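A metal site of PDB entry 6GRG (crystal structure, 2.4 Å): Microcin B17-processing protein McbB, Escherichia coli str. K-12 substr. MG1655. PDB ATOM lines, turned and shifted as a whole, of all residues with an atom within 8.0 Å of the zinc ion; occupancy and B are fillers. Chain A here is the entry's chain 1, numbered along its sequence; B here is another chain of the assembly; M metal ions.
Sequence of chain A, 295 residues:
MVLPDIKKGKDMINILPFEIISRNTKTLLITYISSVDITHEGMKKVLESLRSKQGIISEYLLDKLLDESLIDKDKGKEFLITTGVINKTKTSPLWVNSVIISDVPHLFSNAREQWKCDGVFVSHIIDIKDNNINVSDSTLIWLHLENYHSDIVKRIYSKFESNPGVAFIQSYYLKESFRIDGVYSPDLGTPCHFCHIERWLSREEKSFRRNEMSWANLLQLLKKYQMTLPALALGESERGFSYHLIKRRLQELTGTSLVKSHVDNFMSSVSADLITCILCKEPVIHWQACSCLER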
ATOM      1  N   TYR A 157     -14.950  29.114  10.955  1.00  0.00           N
ATOM      2  CA  TYR A 157     -16.223  29.495  11.599  1.00  0.00           C
ATOM      3  C   TYR A 157     -16.189  29.120  13.077  1.00  0.00           C
ATOM      4  O   TYR A 157     -16.429  29.931  13.956  1.00  0.00           O
ATOM      5  CB  TYR A 157     -17.368  28.814  10.863  1.00  0.00           C
ATOM      6  CG  TYR A 157     -17.718  29.432   9.536  1.00  0.00           C
ATOM      7  CD1 TYR A 157     -16.948  30.446   8.968  1.00  0.00           C
ATOM      8  CD2 TYR A 157     -18.802  28.963   8.808  1.00  0.00           C
ATOM      9  CE1 TYR A 157     -17.275  30.996   7.731  1.00  0.00           C
ATOM     10  CE2 TYR A 157     -19.141  29.511   7.579  1.00  0.00           C
ATOM     11  CZ  TYR A 157     -18.379  30.542   7.043  1.00  0.00           C
ATOM     12  OH  TYR A 157     -18.730  31.084   5.846  1.00  0.00           O
ATOM     13  N   GLU A 161     -16.409  32.574  14.677  1.00  0.00           N
ATOM     14  CA  GLU A 161     -17.820  33.083  14.595  1.00  0.00           C
ATOM     15  C   GLU A 161     -18.200  33.965  15.797  1.00  0.00           C
ATOM     16  O   GLU A 161     -18.969  34.921  15.639  1.00  0.00           O
ATOM     17  CB  GLU A 161     -18.834  31.950  14.532  1.00  0.00           C
ATOM     18  CG  GLU A 161     -19.188  31.547  13.116  1.00  0.00           C
ATOM     19  CD  GLU A 161     -20.222  30.433  13.068  1.00  0.00           C
ATOM     20  OE1 GLU A 161     -20.398  29.730  14.109  1.00  0.00           O
ATOM     21  OE2 GLU A 161     -20.848  30.273  11.980  1.00  0.00           O
ATOM     22  N   TYR A 184     -20.057  37.075   4.942  1.00  0.00           N
ATOM     23  CA  TYR A 184     -20.719  36.359   5.992  1.00  0.00           C
ATOM     24  C   TYR A 184     -20.486  37.125   7.283  1.00  0.00           C
ATOM     25  O   TYR A 184     -19.352  37.187   7.766  1.00  0.00           O
ATOM     26  CB  TYR A 184     -20.242  34.898   6.064  1.00  0.00           C
ATOM     27  CG  TYR A 184     -20.774  34.186   7.279  1.00  0.00           C
ATOM     28  CD1 TYR A 184     -22.093  34.367   7.672  1.00  0.00           C
ATOM     29  CD2 TYR A 184     -19.974  33.389   8.085  1.00  0.00           C
ATOM     30  CE1 TYR A 184     -22.591  33.796   8.825  1.00  0.00           C
ATOM     31  CE2 TYR A 184     -20.459  32.798   9.239  1.00  0.00           C
ATOM     32  CZ  TYR A 184     -21.790  32.989   9.605  1.00  0.00           C
ATOM     33  OH  TYR A 184     -22.314  32.392  10.712  1.00  0.00           O
ATOM     34  N   THR A 190     -26.168  37.588   7.465  1.00  0.00           N
ATOM     35  CA  THR A 190     -25.997  37.279   6.056  1.00  0.00           C
ATOM     36  C   THR A 190     -25.613  35.820   5.839  1.00  0.00           C
ATOM     37  O   THR A 190     -24.969  35.191   6.667  1.00  0.00           O
ATOM     38  CB  THR A 190     -24.972  38.199   5.365  1.00  0.00           C
ATOM     39  OG1 THR A 190     -23.704  38.000   5.970  1.00  0.00           O
ATOM     40  CG2 THR A 190     -25.335  39.661   5.422  1.00  0.00           C
ATOM     41  N   PRO A 191     -25.949  35.249   4.668  1.00  0.00           N
ATOM     42  CA  PRO A 191     -25.634  33.853   4.406  1.00  0.00           C
ATOM     43  C   PRO A 191     -24.147  33.526   4.472  1.00  0.00           C
ATOM     44  O   PRO A 191     -23.334  34.312   4.030  1.00  0.00           O
ATOM     45  CB  PRO A 191     -26.163  33.642   2.979  1.00  0.00           C
ATOM     46  CG  PRO A 191     -27.242  34.687   2.835  1.00  0.00           C
ATOM     47  CD  PRO A 191     -26.682  35.892   3.562  1.00  0.00           C
ATOM     48  N   CYS A 192     -23.854  32.327   4.970  1.00  0.00           N
ATOM     49  CA  CYS A 192     -22.502  31.811   5.165  1.00  0.00           C
ATOM     50  C   CYS A 192     -22.009  31.084   3.907  1.00  0.00           C
ATOM     51  O   CYS A 192     -22.732  30.951   2.926  1.00  0.00           O
ATOM     52  CB  CYS A 192     -22.506  30.860   6.363  1.00  0.00           C
ATOM     53  SG  CYS A 192     -23.210  29.223   5.965  1.00  0.00           S
ATOM     54  N   HIS A 193     -20.775  30.563   3.953  1.00  0.00           N
ATOM     55  CA  HIS A 193     -20.186  29.773   2.856  1.00  0.00           C
ATOM     56  C   HIS A 193     -21.137  28.668   2.372  1.00  0.00           C
ATOM     57  O   HIS A 193     -21.357  28.518   1.197  1.00  0.00           O
ATOM     58  CB  HIS A 193     -18.880  29.100   3.281  1.00  0.00           C
ATOM     59  CG  HIS A 193     -18.379  28.125   2.270  1.00  0.00           C
ATOM     60  ND1 HIS A 193     -17.954  28.517   1.010  1.00  0.00           N
ATOM     61  CD2 HIS A 193     -18.186  26.788   2.328  1.00  0.00           C
ATOM     62  CE1 HIS A 193     -17.532  27.459   0.342  1.00  0.00           C
ATOM     63  NE2 HIS A 193     -17.644  26.382   1.118  1.00  0.00           N
ATOM     64  N   PHE A 194     -21.700  27.897   3.311  1.00  0.00           N
ATOM     65  CA  PHE A 194     -22.423  26.692   2.943  1.00  0.00           C
ATOM     66  C   PHE A 194     -23.734  27.112   2.261  1.00  0.00           C
ATOM     67  O   PHE A 194     -24.262  26.372   1.408  1.00  0.00           O
ATOM     68  CB  PHE A 194     -22.597  25.760   4.138  1.00  0.00           C
ATOM     69  CG  PHE A 194     -21.297  25.292   4.740  1.00  0.00           C
ATOM     70  CD1 PHE A 194     -20.568  24.286   4.129  1.00  0.00           C
ATOM     71  CD2 PHE A 194     -20.799  25.867   5.895  1.00  0.00           C
ATOM     72  CE1 PHE A 194     -19.365  23.872   4.680  1.00  0.00           C
ATOM     73  CE2 PHE A 194     -19.602  25.445   6.449  1.00  0.00           C
ATOM     74  CZ  PHE A 194     -18.880  24.453   5.832  1.00  0.00           C
ATOM     75  N   CYS A 195     -24.250  28.300   2.588  1.00  0.00           N
ATOM     76  CA  CYS A 195     -25.431  28.821   1.896  1.00  0.00           C
ATOM     77  C   CYS A 195     -25.065  29.021   0.421  1.00  0.00           C
ATOM     78  O   CYS A 195     -25.894  28.756  -0.459  1.00  0.00           O
ATOM     79  CB  CYS A 195     -25.956  30.103   2.529  1.00  0.00           C
ATOM     80  SG  CYS A 195     -26.852  29.790   4.072  1.00  0.00           S
ATOM     81  N   HIS A 196     -23.812  29.430   0.173  1.00  0.00           N
ATOM     82  CA  HIS A 196     -23.319  29.730  -1.152  1.00  0.00           C
ATOM     83  C   HIS A 196     -23.087  28.448  -1.947  1.00  0.00           C
ATOM     84  O   HIS A 196     -23.660  28.274  -3.048  1.00  0.00           O
ATOM     85  CB  HIS A 196     -22.080  30.642  -1.101  1.00  0.00           C
ATOM     86  CG  HIS A 196     -22.455  32.055  -0.796  1.00  0.00           C
ATOM     87  ND1 HIS A 196     -22.660  32.499   0.487  1.00  0.00           N
ATOM     88  CD2 HIS A 196     -22.723  33.112  -1.601  1.00  0.00           C
ATOM     89  CE1 HIS A 196     -23.010  33.773   0.460  1.00  0.00           C
ATOM     90  NE2 HIS A 196     -23.061  34.176  -0.808  1.00  0.00           N
ATOM     91  N   ILE A 285     -29.695  33.397  -1.314  1.00  0.00           N
ATOM     92  CA  ILE A 285     -30.621  33.228  -0.167  1.00  0.00           C
ATOM     93  C   ILE A 285     -29.999  32.307   0.902  1.00  0.00           C
ATOM     94  O   ILE A 285     -29.084  31.529   0.652  1.00  0.00           O
ATOM     95  CB  ILE A 285     -31.981  32.683  -0.634  1.00  0.00           C
ATOM     96  CG1 ILE A 285     -31.886  31.263  -1.197  1.00  0.00           C
ATOM     97  CG2 ILE A 285     -32.619  33.637  -1.640  1.00  0.00           C
ATOM     98  CD1 ILE A 285     -33.216  30.617  -1.484  1.00  0.00           C
ATOM     99  N   HIS A 286     -30.538  32.377   2.112  1.00  0.00           N
ATOM    100  CA  HIS A 286     -30.164  31.389   3.117  1.00  0.00           C
ATOM    101  C   HIS A 286     -30.588  29.995   2.613  1.00  0.00           C
ATOM    102  O   HIS A 286     -31.724  29.836   2.100  1.00  0.00           O
ATOM    103  CB  HIS A 286     -30.798  31.754   4.461  1.00  0.00           C
ATOM    104  CG  HIS A 286     -30.193  32.935   5.131  1.00  0.00           C
ATOM    105  ND1 HIS A 286     -30.762  34.202   5.049  1.00  0.00           N
ATOM    106  CD2 HIS A 286     -29.088  33.062   5.907  1.00  0.00           C
ATOM    107  CE1 HIS A 286     -30.021  35.048   5.748  1.00  0.00           C
ATOM    108  NE2 HIS A 286     -28.995  34.360   6.293  1.00  0.00           N
ATOM    109  N   TRP A 287     -29.688  29.012   2.751  1.00  0.00           N
ATOM    110  CA  TRP A 287     -30.000  27.608   2.510  1.00  0.00           C
ATOM    111  C   TRP A 287     -30.860  27.052   3.658  1.00  0.00           C
ATOM    112  O   TRP A 287     -30.546  27.246   4.844  1.00  0.00           O
ATOM    113  CB  TRP A 287     -28.712  26.799   2.340  1.00  0.00           C
ATOM    114  CG  TRP A 287     -28.895  25.332   2.079  1.00  0.00           C
ATOM    115  CD1 TRP A 287     -29.816  24.749   1.254  1.00  0.00           C
ATOM    116  CD2 TRP A 287     -28.098  24.263   2.613  1.00  0.00           C
ATOM    117  NE1 TRP A 287     -29.642  23.381   1.263  1.00  0.00           N
ATOM    118  CE2 TRP A 287     -28.593  23.061   2.073  1.00  0.00           C
ATOM    119  CE3 TRP A 287     -27.001  24.211   3.492  1.00  0.00           C
ATOM    120  CZ2 TRP A 287     -28.043  21.824   2.402  1.00  0.00           C
ATOM    121  CZ3 TRP A 287     -26.452  22.982   3.810  1.00  0.00           C
ATOM    122  CH2 TRP A 287     -26.983  21.804   3.273  1.00  0.00           C
ATOM    123  N   GLN A 288     -31.933  26.341   3.298  1.00  0.00           N
ATOM    124  CA  GLN A 288     -32.978  25.937   4.243  1.00  0.00           C
ATOM    125  C   GLN A 288     -32.408  24.955   5.295  1.00  0.00           C
ATOM    126  O   GLN A 288     -32.881  24.906   6.428  1.00  0.00           O
ATOM    127  CB  GLN A 288     -34.178  25.354   3.479  1.00  0.00           C
ATOM    128  CG  GLN A 288     -33.858  24.135   2.603  1.00  0.00           C
ATOM    129  CD  GLN A 288     -34.977  23.818   1.628  1.00  0.00           C
ATOM    130  OE1 GLN A 288     -36.117  24.314   1.735  1.00  0.00           O
ATOM    131  NE2 GLN A 288     -34.657  22.976   0.666  1.00  0.00           N
ATOM    132  N   ALA A 289     -31.413  24.161   4.904  1.00  0.00           N
ATOM    133  CA  ALA A 289     -30.904  23.138   5.740  1.00  0.00           C
ATOM    134  C   ALA A 289     -29.660  23.627   6.491  1.00  0.00           C
ATOM    135  O   ALA A 289     -28.961  22.829   7.124  1.00  0.00           O
ATOM    136  CB  ALA A 289     -30.603  21.928   4.889  1.00  0.00           C
ATOM    137  N   CYS A 290     -29.392  24.937   6.439  1.00  0.00           N
ATOM    138  CA  CYS A 290     -28.196  25.479   7.021  1.00  0.00           C
ATOM    139  C   CYS A 290     -28.475  25.942   8.430  1.00  0.00           C
ATOM    140  O   CYS A 290     -29.593  26.281   8.755  1.00  0.00           O
ATOM    141  CB  CYS A 290     -27.674  26.688   6.260  1.00  0.00           C
ATOM    142  SG  CYS A 290     -25.919  27.026   6.536  1.00  0.00           S
ATOM    143  N   SER A 291     -27.390  26.046   9.206  1.00  0.00           N
ATOM    144  CA  SER A 291     -27.426  26.328  10.641  1.00  0.00           C
ATOM    145  C   SER A 291     -27.033  27.773  10.963  1.00  0.00           C
ATOM    146  O   SER A 291     -27.191  28.184  12.101  1.00  0.00           O
ATOM    147  CB  SER A 291     -26.482  25.380  11.349  1.00  0.00           C
ATOM    148  OG  SER A 291     -25.134  25.712  11.054  1.00  0.00           O
ATOM    149  N   CYS A 292     -26.516  28.545   9.982  1.00  0.00           N
ATOM    150  CA  CYS A 292     -25.856  29.820  10.265  1.00  0.00           C
ATOM    151  C   CYS A 292     -26.825  30.835  10.897  1.00  0.00           C
ATOM    152  O   CYS A 292     -26.401  31.710  11.635  1.00  0.00           O
ATOM    153  CB  CYS A 292     -25.135  30.387   9.043  1.00  0.00           C
ATOM    154  SG  CYS A 292     -26.192  30.776   7.608  1.00  0.00           S
ATOM    155  N   LEU A 293     -28.126  30.721  10.624  1.00  0.00           N
ATOM    156  CA  LEU A 293     -29.133  31.609  11.214  1.00  0.00           C
ATOM    157  C   LEU A 293     -29.379  31.298  12.695  1.00  0.00           C
ATOM    158  O   LEU A 293     -29.827  32.195  13.420  1.00  0.00           O
ATOM    159  CB  LEU A 293     -30.462  31.448  10.469  1.00  0.00           C
ATOM    160  CG  LEU A 293     -30.446  31.848   9.007  1.00  0.00           C
ATOM    161  CD1 LEU A 293     -30.619  30.621   8.144  1.00  0.00           C
ATOM    162  CD2 LEU A 293     -31.544  32.863   8.753  1.00  0.00           C
ATOM    163  N   ARG A 295     -27.183  30.158  14.898  1.00  0.00           N
ATOM    164  CA  ARG A 295     -26.036  30.495  15.744  1.00  0.00           C
ATOM    165  C   ARG A 295     -26.237  31.934  16.248  1.00  0.00           C
ATOM    166  O   ARG A 295     -26.602  32.838  15.499  1.00  0.00           O
ATOM    167  CB  ARG A 295     -24.726  30.166  15.005  1.00  0.00           C
ATOM    168  CG  ARG A 295     -24.502  28.650  14.933  1.00  0.00           C
ATOM    169  CD  ARG A 295     -23.119  28.226  14.527  1.00  0.00           C
ATOM    170  NE  ARG A 295     -22.937  28.400  13.105  1.00  0.00           N
ATOM    171  CZ  ARG A 295     -22.422  27.487  12.283  1.00  0.00           C
ATOM    172  NH1 ARG A 295     -22.116  26.285  12.760  1.00  0.00           N
ATOM    173  NH2 ARG A 295     -22.157  27.801  11.009  1.00  0.00           N
ATOM    174  OXT ARG A 295     -26.154  32.231  17.454  1.00  0.00           O
ATOM    175  N   ARG B 252     -35.366  32.363   6.818  1.00  0.00           N
ATOM    176  CA  ARG B 252     -35.832  31.297   5.926  1.00  0.00           C
ATOM    177  C   ARG B 252     -37.362  31.294   5.832  1.00  0.00           C
ATOM    178  O   ARG B 252     -37.925  30.820   4.838  1.00  0.00           O
ATOM    179  CB  ARG B 252     -35.337  29.932   6.418  1.00  0.00           C
ATOM    180  CG  ARG B 252     -33.834  29.711   6.296  1.00  0.00           C
ATOM    181  CD  ARG B 252     -33.312  28.549   7.113  1.00  0.00           C
ATOM    182  NE  ARG B 252     -33.536  28.749   8.540  1.00  0.00           N
ATOM    183  CZ  ARG B 252     -33.257  27.856   9.471  1.00  0.00           C
ATOM    184  NH1 ARG B 252     -32.742  26.685   9.121  1.00  0.00           N
ATOM    185  NH2 ARG B 252     -33.435  28.145  10.750  1.00  0.00           N
HETATM  186 ZN    ZN M   1     -25.522  29.260   5.955  1.00  0.00          ZN
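The zinc ion is bound by the side-chain sulfur (SG) of Cys 192 (2.3 Å), the side-chain sulfur (SG) of Cys 292 (2.3 Å), the side-chain sulfur (SG) of Cys 290 (2.3 Å) and the side-chain sulfur (SG) of Cys 195 (2.4 Å). The zinc ion has four donor atoms within binding distance.
SG of Cys 192 sits close to N of Phe 194 (3.3 Å). A ring nitrogen (ND1) of His 196 is in hydrogen-bond range of the backbone carbonyl oxygen (O) of Cys 192. NH1 of Arg 252 of chain B sits at hydrogen-bond distance from O of Cys 290 (3.2 Å). The backbone NH (N) of Trp 287 sits close to the side-chain sulfur (SG) of Cys 195, 3.2 Å away.
Within 4 Å of the zinc ion: Cys 192, Cys 195, Cys 290 and Cys 292.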
